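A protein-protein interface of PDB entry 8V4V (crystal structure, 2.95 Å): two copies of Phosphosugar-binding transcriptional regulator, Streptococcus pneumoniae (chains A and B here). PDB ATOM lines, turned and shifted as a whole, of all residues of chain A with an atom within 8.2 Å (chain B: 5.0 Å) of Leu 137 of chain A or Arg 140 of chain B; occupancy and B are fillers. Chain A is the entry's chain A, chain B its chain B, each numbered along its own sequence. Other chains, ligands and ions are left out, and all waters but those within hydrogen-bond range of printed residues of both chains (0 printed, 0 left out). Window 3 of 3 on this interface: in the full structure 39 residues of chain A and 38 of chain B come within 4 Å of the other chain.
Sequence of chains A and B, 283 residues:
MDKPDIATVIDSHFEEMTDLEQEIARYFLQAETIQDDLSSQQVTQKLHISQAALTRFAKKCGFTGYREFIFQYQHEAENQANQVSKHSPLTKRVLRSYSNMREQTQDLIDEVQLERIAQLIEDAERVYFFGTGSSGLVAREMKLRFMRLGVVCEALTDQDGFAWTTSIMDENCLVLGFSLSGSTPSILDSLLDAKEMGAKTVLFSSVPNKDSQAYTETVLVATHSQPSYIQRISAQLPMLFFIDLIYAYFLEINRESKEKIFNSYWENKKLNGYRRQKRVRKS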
ATOM      1  N   PHE A 130      -0.122  13.404 -18.078  1.00  0.00           N
ATOM      2  CA  PHE A 130       0.131  12.033 -18.501  1.00  0.00           C
ATOM      3  C   PHE A 130       1.414  11.523 -17.852  1.00  0.00           C
ATOM      4  O   PHE A 130       2.425  12.230 -17.808  1.00  0.00           O
ATOM      5  CB  PHE A 130       0.240  11.934 -20.028  1.00  0.00           C
ATOM      6  CG  PHE A 130      -1.054  12.204 -20.761  1.00  0.00           C
ATOM      7  CD1 PHE A 130      -2.260  12.259 -20.084  1.00  0.00           C
ATOM      8  CD2 PHE A 130      -1.053  12.395 -22.135  1.00  0.00           C
ATOM      9  CE1 PHE A 130      -3.432  12.504 -20.758  1.00  0.00           C
ATOM     10  CE2 PHE A 130      -2.224  12.641 -22.815  1.00  0.00           C
ATOM     11  CZ  PHE A 130      -3.414  12.694 -22.127  1.00  0.00           C
ATOM     12  N   GLY A 131       1.361  10.299 -17.340  1.00  0.00           N
ATOM     13  CA  GLY A 131       2.526   9.690 -16.729  1.00  0.00           C
ATOM     14  C   GLY A 131       2.296   8.212 -16.517  1.00  0.00           C
ATOM     15  O   GLY A 131       1.157   7.741 -16.486  1.00  0.00           O
ATOM     16  N   THR A 132       3.400   7.484 -16.374  1.00  0.00           N
ATOM     17  CA  THR A 132       3.356   6.043 -16.186  1.00  0.00           C
ATOM     18  C   THR A 132       4.226   5.648 -15.001  1.00  0.00           C
ATOM     19  O   THR A 132       5.231   6.298 -14.702  1.00  0.00           O
ATOM     20  CB  THR A 132       3.825   5.288 -17.440  1.00  0.00           C
ATOM     21  OG1 THR A 132       5.112   5.772 -17.843  1.00  0.00           O
ATOM     22  CG2 THR A 132       2.838   5.476 -18.580  1.00  0.00           C
ATOM     23  N   GLY A 133       3.824   4.575 -14.329  1.00  0.00           N
ATOM     24  CA  GLY A 133       4.583   4.101 -13.184  1.00  0.00           C
ATOM     25  C   GLY A 133       4.699   5.178 -12.125  1.00  0.00           C
ATOM     26  O   GLY A 133       3.712   5.808 -11.733  1.00  0.00           O
ATOM     27  N   SER A 134       5.923   5.392 -11.642  1.00  0.00           N
ATOM     28  CA  SER A 134       6.150   6.450 -10.664  1.00  0.00           C
ATOM     29  C   SER A 134       5.952   7.831 -11.277  1.00  0.00           C
ATOM     30  O   SER A 134       5.503   8.755 -10.589  1.00  0.00           O
ATOM     31  CB  SER A 134       7.552   6.322 -10.072  1.00  0.00           C
ATOM     32  OG  SER A 134       7.526   5.604  -8.851  1.00  0.00           O
ATOM     33  N   SER A 135       6.293   7.997 -12.557  1.00  0.00           N
ATOM     34  CA  SER A 135       5.968   9.237 -13.250  1.00  0.00           C
ATOM     35  C   SER A 135       4.464   9.472 -13.310  1.00  0.00           C
ATOM     36  O   SER A 135       4.030  10.621 -13.473  1.00  0.00           O
ATOM     37  CB  SER A 135       6.549   9.217 -14.663  1.00  0.00           C
ATOM     38  OG  SER A 135       7.844   9.787 -14.688  1.00  0.00           O
ATOM     39  N   GLY A 136       3.667   8.409 -13.203  1.00  0.00           N
ATOM     40  CA  GLY A 136       2.225   8.530 -13.144  1.00  0.00           C
ATOM     41  C   GLY A 136       1.748   9.014 -11.792  1.00  0.00           C
ATOM     42  O   GLY A 136       0.845   9.848 -11.711  1.00  0.00           O
ATOM     43  N   LEU A 137       2.351   8.498 -10.718  1.00  0.00           N
ATOM     44  CA  LEU A 137       2.031   9.005  -9.390  1.00  0.00           C
ATOM     45  C   LEU A 137       2.334  10.492  -9.291  1.00  0.00           C
ATOM     46  O   LEU A 137       1.619  11.228  -8.602  1.00  0.00           O
ATOM     47  CB  LEU A 137       2.809   8.232  -8.326  1.00  0.00           C
ATOM     48  CG  LEU A 137       2.576   6.721  -8.265  1.00  0.00           C
ATOM     49  CD1 LEU A 137       3.554   6.094  -7.282  1.00  0.00           C
ATOM     50  CD2 LEU A 137       1.144   6.404  -7.880  1.00  0.00           C
ATOM     51  N   VAL A 138       3.385  10.950  -9.977  1.00  0.00           N
ATOM     52  CA  VAL A 138       3.700  12.375 -10.009  1.00  0.00           C
ATOM     53  C   VAL A 138       2.584  13.146 -10.700  1.00  0.00           C
ATOM     54  O   VAL A 138       2.235  14.263 -10.297  1.00  0.00           O
ATOM     55  CB  VAL A 138       5.057  12.598 -10.703  1.00  0.00           C
ATOM     56  CG1 VAL A 138       5.094  13.964 -11.366  1.00  0.00           C
ATOM     57  CG2 VAL A 138       6.191  12.451  -9.706  1.00  0.00           C
ATOM     58  N   ALA A 139       2.025  12.576 -11.766  1.00  0.00           N
ATOM     59  CA  ALA A 139       0.900  13.220 -12.432  1.00  0.00           C
ATOM     60  C   ALA A 139      -0.331  13.243 -11.536  1.00  0.00           C
ATOM     61  O   ALA A 139      -1.101  14.211 -11.559  1.00  0.00           O
ATOM     62  CB  ALA A 139       0.588  12.507 -13.745  1.00  0.00           C
ATOM     63  N   ARG A 140      -0.548  12.179 -10.757  1.00  0.00           N
ATOM     64  CA  ARG A 140      -1.718  12.127  -9.884  1.00  0.00           C
ATOM     65  C   ARG A 140      -1.686  13.252  -8.855  1.00  0.00           C
ATOM     66  O   ARG A 140      -2.689  13.942  -8.640  1.00  0.00           O
ATOM     67  CB  ARG A 140      -1.805  10.766  -9.181  1.00  0.00           C
ATOM     68  CG  ARG A 140      -1.742   9.544 -10.095  1.00  0.00           C
ATOM     69  CD  ARG A 140      -3.120   9.197 -10.666  1.00  0.00           C
ATOM     70  NE  ARG A 140      -3.764   8.027 -10.073  1.00  0.00           N
ATOM     71  CZ  ARG A 140      -3.373   6.773 -10.261  1.00  0.00           C
ATOM     72  NH1 ARG A 140      -2.235   6.488 -10.872  1.00  0.00           N
ATOM     73  NH2 ARG A 140      -4.141   5.780  -9.824  1.00  0.00           N
ATOM     74  N   GLU A 141      -0.539  13.447  -8.197  1.00  0.00           N
ATOM     75  CA  GLU A 141      -0.466  14.489  -7.178  1.00  0.00           C
ATOM     76  C   GLU A 141      -0.682  15.867  -7.786  1.00  0.00           C
ATOM     77  O   GLU A 141      -1.392  16.700  -7.211  1.00  0.00           O
ATOM     78  CB  GLU A 141       0.873  14.456  -6.442  1.00  0.00           C
ATOM     79  CG  GLU A 141       1.130  15.745  -5.648  1.00  0.00           C
ATOM     80  CD  GLU A 141       1.888  15.526  -4.345  1.00  0.00           C
ATOM     81  OE1 GLU A 141       3.102  15.241  -4.387  1.00  0.00           O
ATOM     82  OE2 GLU A 141       1.267  15.644  -3.269  1.00  0.00           O
ATOM     83  N   MET A 142      -0.067  16.136  -8.940  1.00  0.00           N
ATOM     84  CA  MET A 142      -0.200  17.457  -9.543  1.00  0.00           C
ATOM     85  C   MET A 142      -1.660  17.782  -9.827  1.00  0.00           C
ATOM     86  O   MET A 142      -2.118  18.898  -9.562  1.00  0.00           O
ATOM     87  CB  MET A 142       0.628  17.541 -10.823  1.00  0.00           C
ATOM     88  CG  MET A 142       1.156  18.940 -11.098  1.00  0.00           C
ATOM     89  SD  MET A 142       1.856  19.157 -12.741  1.00  0.00           S
ATOM     90  CE  MET A 142       2.672  20.742 -12.541  1.00  0.00           C
ATOM     91  N   LYS A 143      -2.409  16.819 -10.363  1.00  0.00           N
ATOM     92  CA  LYS A 143      -3.841  17.023 -10.538  1.00  0.00           C
ATOM     93  C   LYS A 143      -4.494  17.419  -9.220  1.00  0.00           C
ATOM     94  O   LYS A 143      -5.258  18.390  -9.157  1.00  0.00           O
ATOM     95  CB  LYS A 143      -4.483  15.754 -11.093  1.00  0.00           C
ATOM     96  CG  LYS A 143      -5.935  15.924 -11.503  1.00  0.00           C
ATOM     97  CD  LYS A 143      -6.872  15.136 -10.592  1.00  0.00           C
ATOM     98  CE  LYS A 143      -8.336  15.383 -10.949  1.00  0.00           C
ATOM     99  NZ  LYS A 143      -8.731  16.804 -10.736  1.00  0.00           N
ATOM    100  N   LEU A 144      -4.199  16.678  -8.150  1.00  0.00           N
ATOM    101  CA  LEU A 144      -4.780  17.004  -6.854  1.00  0.00           C
ATOM    102  C   LEU A 144      -4.431  18.430  -6.444  1.00  0.00           C
ATOM    103  O   LEU A 144      -5.314  19.219  -6.107  1.00  0.00           O
ATOM    104  CB  LEU A 144      -4.308  16.004  -5.798  1.00  0.00           C
ATOM    105  CG  LEU A 144      -5.303  14.905  -5.418  1.00  0.00           C
ATOM    106  CD1 LEU A 144      -5.863  14.228  -6.658  1.00  0.00           C
ATOM    107  CD2 LEU A 144      -4.653  13.892  -4.490  1.00  0.00           C
ATOM    108  N   ALA A 155      -5.790  13.532 -14.607  1.00  0.00           N
ATOM    109  CA  ALA A 155      -4.564  12.750 -14.670  1.00  0.00           C
ATOM    110  C   ALA A 155      -4.881  11.392 -15.283  1.00  0.00           C
ATOM    111  O   ALA A 155      -5.865  10.749 -14.902  1.00  0.00           O
ATOM    112  CB  ALA A 155      -3.943  12.586 -13.280  1.00  0.00           C
ATOM    113  N   LEU A 156      -4.059  10.969 -16.237  1.00  0.00           N
ATOM    114  CA  LEU A 156      -4.247   9.712 -16.947  1.00  0.00           C
ATOM    115  C   LEU A 156      -2.931   8.956 -16.952  1.00  0.00           C
ATOM    116  O   LEU A 156      -1.865   9.559 -17.102  1.00  0.00           O
ATOM    117  CB  LEU A 156      -4.738   9.968 -18.373  1.00  0.00           C
ATOM    118  CG  LEU A 156      -6.115  10.641 -18.389  1.00  0.00           C
ATOM    119  CD1 LEU A 156      -6.009  12.137 -18.648  1.00  0.00           C
ATOM    120  CD2 LEU A 156      -7.034   9.982 -19.410  1.00  0.00           C
ATOM    121  N   THR A 157      -3.003   7.631 -16.780  1.00  0.00           N
ATOM    122  CA  THR A 157      -1.795   6.833 -16.612  1.00  0.00           C
ATOM    123  C   THR A 157      -1.788   5.573 -17.472  1.00  0.00           C
ATOM    124  O   THR A 157      -1.049   4.632 -17.165  1.00  0.00           O
ATOM    125  CB  THR A 157      -1.602   6.440 -15.143  1.00  0.00           C
ATOM    126  OG1 THR A 157      -2.865   6.081 -14.564  1.00  0.00           O
ATOM    127  CG2 THR A 157      -0.985   7.589 -14.355  1.00  0.00           C
ATOM    128  N   PHE A 178       4.988  13.327 -18.350  1.00  0.00           N
ATOM    129  CA  PHE A 178       5.990  12.968 -17.351  1.00  0.00           C
ATOM    130  C   PHE A 178       6.615  11.638 -17.739  1.00  0.00           C
ATOM    131  O   PHE A 178       5.948  10.600 -17.705  1.00  0.00           O
ATOM    132  CB  PHE A 178       5.366  12.894 -15.959  1.00  0.00           C
ATOM    133  CG  PHE A 178       5.040  14.239 -15.377  1.00  0.00           C
ATOM    134  CD1 PHE A 178       6.051  15.055 -14.897  1.00  0.00           C
ATOM    135  CD2 PHE A 178       3.732  14.701 -15.322  1.00  0.00           C
ATOM    136  CE1 PHE A 178       5.771  16.309 -14.359  1.00  0.00           C
ATOM    137  CE2 PHE A 178       3.441  15.962 -14.786  1.00  0.00           C
ATOM    138  CZ  PHE A 178       4.466  16.765 -14.304  1.00  0.00           C
ATOM    139  N   SER A 234      13.453   7.436  -4.714  1.00  0.00           N
ATOM    140  CA  SER A 234      12.173   7.505  -5.411  1.00  0.00           C
ATOM    141  C   SER A 234      12.318   8.194  -6.761  1.00  0.00           C
ATOM    142  O   SER A 234      12.988   9.223  -6.880  1.00  0.00           O
ATOM    143  CB  SER A 234      11.148   8.255  -4.556  1.00  0.00           C
ATOM    144  OG  SER A 234      10.189   8.913  -5.364  1.00  0.00           O
ATOM    145  N   GLN A 236      10.054   9.736  -8.344  1.00  0.00           N
ATOM    146  CA  GLN A 236       9.204  10.909  -8.490  1.00  0.00           C
ATOM    147  C   GLN A 236       9.979  12.198  -8.257  1.00  0.00           C
ATOM    148  O   GLN A 236       9.613  13.248  -8.797  1.00  0.00           O
ATOM    149  CB  GLN A 236       8.039  10.856  -7.503  1.00  0.00           C
ATOM    150  CG  GLN A 236       7.137   9.648  -7.596  1.00  0.00           C
ATOM    151  CD  GLN A 236       5.895   9.804  -6.736  1.00  0.00           C
ATOM    152  OE1 GLN A 236       4.867  10.309  -7.188  1.00  0.00           O
ATOM    153  NE2 GLN A 236       5.998   9.400  -5.476  1.00  0.00           N
ATOM    154  N   LEU A 240       8.946  16.171  -8.708  1.00  0.00           N
ATOM    155  CA  LEU A 240       8.230  16.868  -7.647  1.00  0.00           C
ATOM    156  C   LEU A 240       8.915  18.178  -7.289  1.00  0.00           C
ATOM    157  O   LEU A 240       8.263  19.104  -6.797  1.00  0.00           O
ATOM    158  CB  LEU A 240       8.118  15.974  -6.417  1.00  0.00           C
ATOM    159  CG  LEU A 240       7.282  14.703  -6.563  1.00  0.00           C
ATOM    160  CD1 LEU A 240       7.446  13.841  -5.321  1.00  0.00           C
ATOM    161  CD2 LEU A 240       5.817  15.036  -6.800  1.00  0.00           C
ATOM    162  N   ILE A 243       7.449  20.509 -10.007  1.00  0.00           N
ATOM    163  CA  ILE A 243       6.021  20.694  -9.773  1.00  0.00           C
ATOM    164  C   ILE A 243       5.802  21.729  -8.676  1.00  0.00           C
ATOM    165  O   ILE A 243       4.974  22.637  -8.805  1.00  0.00           O
ATOM    166  CB  ILE A 243       5.351  19.355  -9.421  1.00  0.00           C
ATOM    167  CG1 ILE A 243       5.155  18.518 -10.683  1.00  0.00           C
ATOM    168  CG2 ILE A 243       4.013  19.602  -8.726  1.00  0.00           C
ATOM    169  CD1 ILE A 243       4.715  17.114 -10.403  1.00  0.00           C
ATOM    170  N   GLY B 136      -1.955   8.529  -0.004  1.00  0.00           N
ATOM    171  CA  GLY B 136      -2.258   7.376  -0.834  1.00  0.00           C
ATOM    172  C   GLY B 136      -1.220   7.144  -1.914  1.00  0.00           C
ATOM    173  O   GLY B 136      -0.843   6.001  -2.189  1.00  0.00           O
ATOM    174  N   LEU B 137      -0.746   8.222  -2.546  1.00  0.00           N
ATOM    175  CA  LEU B 137       0.299   8.085  -3.555  1.00  0.00           C
ATOM    176  C   LEU B 137       1.554   7.481  -2.946  1.00  0.00           C
ATOM    177  O   LEU B 137       2.208   6.629  -3.559  1.00  0.00           O
ATOM    178  CB  LEU B 137       0.610   9.443  -4.180  1.00  0.00           C
ATOM    179  CG  LEU B 137      -0.602  10.169  -4.755  1.00  0.00           C
ATOM    180  CD1 LEU B 137      -0.202  11.532  -5.267  1.00  0.00           C
ATOM    181  CD2 LEU B 137      -1.241   9.349  -5.864  1.00  0.00           C
ATOM    182  N   VAL B 138       1.893   7.903  -1.726  1.00  0.00           N
ATOM    183  CA  VAL B 138       3.050   7.348  -1.033  1.00  0.00           C
ATOM    184  C   VAL B 138       2.889   5.845  -0.853  1.00  0.00           C
ATOM    185  O   VAL B 138       3.828   5.074  -1.085  1.00  0.00           O
ATOM    186  CB  VAL B 138       3.250   8.063   0.317  1.00  0.00           C
ATOM    187  CG1 VAL B 138       4.006   7.163   1.290  1.00  0.00           C
ATOM    188  CG2 VAL B 138       3.977   9.385   0.111  1.00  0.00           C
ATOM    189  N   ALA B 139       1.701   5.404  -0.434  1.00  0.00           N
ATOM    190  CA  ALA B 139       1.464   3.976  -0.249  1.00  0.00           C
ATOM    191  C   ALA B 139       1.534   3.227  -1.575  1.00  0.00           C
ATOM    192  O   ALA B 139       2.022   2.090  -1.629  1.00  0.00           O
ATOM    193  CB  ALA B 139       0.108   3.763   0.423  1.00  0.00           C
ATOM    194  N   ARG B 140       1.039   3.837  -2.653  1.00  0.00           N
ATOM    195  CA  ARG B 140       1.101   3.186  -3.957  1.00  0.00           C
ATOM    196  C   ARG B 140       2.540   3.021  -4.430  1.00  0.00           C
ATOM    197  O   ARG B 140       2.911   1.955  -4.935  1.00  0.00           O
ATOM    198  CB  ARG B 140       0.290   3.979  -4.978  1.00  0.00           C
ATOM    199  CG  ARG B 140      -1.106   3.427  -5.218  1.00  0.00           C
ATOM    200  CD  ARG B 140      -1.935   4.383  -6.068  1.00  0.00           C
ATOM    201  NE  ARG B 140      -2.749   5.277  -5.253  1.00  0.00           N
ATOM    202  CZ  ARG B 140      -3.817   5.934  -5.688  1.00  0.00           C
ATOM    203  NH1 ARG B 140      -4.239   5.818  -6.938  1.00  0.00           N
ATOM    204  NH2 ARG B 140      -4.478   6.727  -4.846  1.00  0.00           N
ATOM    205  N   GLU B 141       3.370   4.058  -4.271  1.00  0.00           N
ATOM    206  CA  GLU B 141       4.758   3.953  -4.712  1.00  0.00           C
ATOM    207  C   GLU B 141       5.498   2.875  -3.931  1.00  0.00           C
ATOM    208  O   GLU B 141       6.301   2.126  -4.500  1.00  0.00           O
ATOM    209  CB  GLU B 141       5.478   5.295  -4.575  1.00  0.00           C
ATOM    210  CG  GLU B 141       6.564   5.493  -5.635  1.00  0.00           C
ATOM    211  CD  GLU B 141       7.732   6.341  -5.157  1.00  0.00           C
ATOM    212  OE1 GLU B 141       8.044   6.321  -3.947  1.00  0.00           O
ATOM    213  OE2 GLU B 141       8.358   7.009  -6.008  1.00  0.00           O
ATOM    214  N   MET B 142       5.241   2.778  -2.624  1.00  0.00           N
ATOM    215  CA  MET B 142       5.889   1.738  -1.832  1.00  0.00           C
ATOM    216  C   MET B 142       5.503   0.353  -2.337  1.00  0.00           C
ATOM    217  O   MET B 142       6.341  -0.558  -2.367  1.00  0.00           O
ATOM    218  CB  MET B 142       5.530   1.893  -0.354  1.00  0.00           C
ATOM    219  CG  MET B 142       6.687   1.552   0.579  1.00  0.00           C
ATOM    220  SD  MET B 142       6.237   1.423   2.319  1.00  0.00           S
ATOM    221  CE  MET B 142       7.839   1.094   3.050  1.00  0.00           C
ATOM    222  N   LYS B 143       4.237   0.173  -2.725  1.00  0.00           N
ATOM    223  CA  LYS B 143       3.811  -1.096  -3.306  1.00  0.00           C
ATOM    224  C   LYS B 143       4.572  -1.380  -4.592  1.00  0.00           C
ATOM    225  O   LYS B 143       5.085  -2.487  -4.800  1.00  0.00           O
ATOM    226  CB  LYS B 143       2.306  -1.070  -3.579  1.00  0.00           C
ATOM    227  CG  LYS B 143       1.682  -2.445  -3.759  1.00  0.00           C
ATOM    228  CD  LYS B 143       1.598  -2.852  -5.222  1.00  0.00           C
ATOM    229  CE  LYS B 143       0.976  -4.236  -5.349  1.00  0.00           C
ATOM    230  NZ  LYS B 143       1.082  -4.817  -6.714  1.00  0.00           N
ATOM    231  N   LEU B 144       4.676  -0.374  -5.462  1.00  0.00           N
ATOM    232  CA  LEU B 144       5.369  -0.555  -6.729  1.00  0.00           C
ATOM    233  C   LEU B 144       6.836  -0.880  -6.513  1.00  0.00           C
ATOM    234  O   LEU B 144       7.403  -1.693  -7.243  1.00  0.00           O
ATOM    235  CB  LEU B 144       5.212   0.700  -7.590  1.00  0.00           C
ATOM    236  CG  LEU B 144       5.915   0.797  -8.947  1.00  0.00           C
ATOM    237  CD1 LEU B 144       5.118   1.779  -9.811  1.00  0.00           C
ATOM    238  CD2 LEU B 144       7.351   1.257  -8.814  1.00  0.00           C
ATOM    239  N   ALA B 155      -1.821  -2.046  -2.051  1.00  0.00           N
ATOM    240  CA  ALA B 155      -1.961  -0.666  -1.609  1.00  0.00           C
ATOM    241  C   ALA B 155      -3.425  -0.275  -1.700  1.00  0.00           C
ATOM    242  O   ALA B 155      -4.066  -0.505  -2.730  1.00  0.00           O
ATOM    243  CB  ALA B 155      -1.110   0.284  -2.451  1.00  0.00           C
ATOM    244  N   THR B 157      -6.579   2.720  -0.662  1.00  0.00           N
ATOM    245  CA  THR B 157      -6.743   4.160  -0.511  1.00  0.00           C
ATOM    246  C   THR B 157      -8.201   4.572  -0.341  1.00  0.00           C
ATOM    247  O   THR B 157      -8.545   5.722  -0.638  1.00  0.00           O
ATOM    248  CB  THR B 157      -6.154   4.899  -1.725  1.00  0.00           C
ATOM    249  OG1 THR B 157      -6.345   6.316  -1.586  1.00  0.00           O
ATOM    250  CG2 THR B 157      -6.817   4.404  -3.017  1.00  0.00           C
ATOM    251  N   GLN B 236       3.875  14.487   0.074  1.00  0.00           N
ATOM    252  CA  GLN B 236       4.417  13.135   0.012  1.00  0.00           C
ATOM    253  C   GLN B 236       5.789  13.025   0.664  1.00  0.00           C
ATOM    254  O   GLN B 236       6.141  11.958   1.182  1.00  0.00           O
ATOM    255  CB  GLN B 236       4.523  12.673  -1.444  1.00  0.00           C
ATOM    256  CG  GLN B 236       3.199  12.505  -2.167  1.00  0.00           C
ATOM    257  CD  GLN B 236       3.344  11.714  -3.456  1.00  0.00           C
ATOM    258  OE1 GLN B 236       3.654  10.523  -3.435  1.00  0.00           O
ATOM    259  NE2 GLN B 236       3.136  12.378  -4.588  1.00  0.00           N
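Among the printed residues, pairs that only touch across the chains: Glu 141 of chain A with Leu 137 of chain B (3.3 Å), Leu 137 of chain A with Glu 141 of chain B (3.4 Å), Arg 140 of chain A with Leu 137 of chain B (3.7 Å), Leu 137 of chain A with Leu 137 of chain B (3.8 Å) and Leu 137 of chain A with Arg 140 of chain B (3.9 Å).
Hydrophobic or aromatic side chains of chain A within 4 Å of the printed part of chain B: Leu 137. Of the 12 printed residues of chain B, 4 touch a printed residue of chain A. Along chain B the printed residues that touch a printed residue of chain A span positions 137 to 236.
OE1 of Gln 236 of chain A sits at hydrogen-bond distance from N of Val 138 of chain A. The side-chain hydroxyl (OG) of Ser 234 of chain A lies within hydrogen-bond range of the backbone NH (N) of Gln 236 of chain A, at 3.1 Å.
Leu 137 of chain A touches its own counterpart, Leu 137 of chain B. Leu 137 of chain A touches Glu 141 of chain B, and with the chains exchanged Glu 141 of chain A touches Leu 137 of chain B. Arg 140 of chain B touches its own counterpart, Arg 140 of chain A. Gln 236 of chain B touches its own counterpart, Gln 236 of chain A. Of the 11 pairs that touch across the chains among the printed residues, 9 have their exchanged pair printed and touching as well.
OE2 of Glu 141 of chain B is in hydrogen-bond range of OG of Ser 134 of chain A. The side-chain hydroxyl (OG) of Ser 234 of chain A sits at hydrogen-bond distance from the side-chain carboxylate (OE2) of Glu 141 of chain B (2.7 Å). OE2 of Glu 141 of chain B sits close to NE2 of Gln 236 of chain A (3.4 Å). The side-chain carboxylate (OE1) of Glu 141 of chain A sits at hydrogen-bond distance from the side-chain amide nitrogen (NE2) of Gln 236 of chain B (2.9 Å). The side-chain amide oxygen (OE1) of Gln 236 of chain B sits at hydrogen-bond distance from the side-chain amide nitrogen (NE2) of Gln 236 of chain A (3.3 Å). The guanidinium group of Arg 140 of chain A sits close to the guanidinium group of Arg 140 of chain B (2.9 Å).
Printed residues of chain B within 4 Å of Ser 134 of chain A: Glu 141. Of chain B, only Leu 137, Arg 140 and Glu 141 come within 4 Å of Leu 137 of chain A. Printed residues of chain B within 4 Å of Arg 140 of chain A: Leu 137 and Arg 140. Printed residues of chain B within 4 Å of Glu 141 of chain A: Leu 137 (3.3 Å) and Gln 236 (2.9 Å). Printed residues of chain B within 4 Å of Ser 234 of chain A: Glu 141. Ala 139 of chain B touches none of the printed residues of chain A. Arg 140 of chain B touches just these residues of chain A: Leu 137 (3.9 Å) and Arg 140 (2.9 Å). Leu 144 of chain B touches none of the printed residues of chain A. The nearest residue of chain A that does not touch Arg 140 of chain B is Ser 134 of chain A (7.1 Å). The nearest printed residue of chain A that does not touch Leu 137 of chain B is Gln 236 of chain A (5.1 Å).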
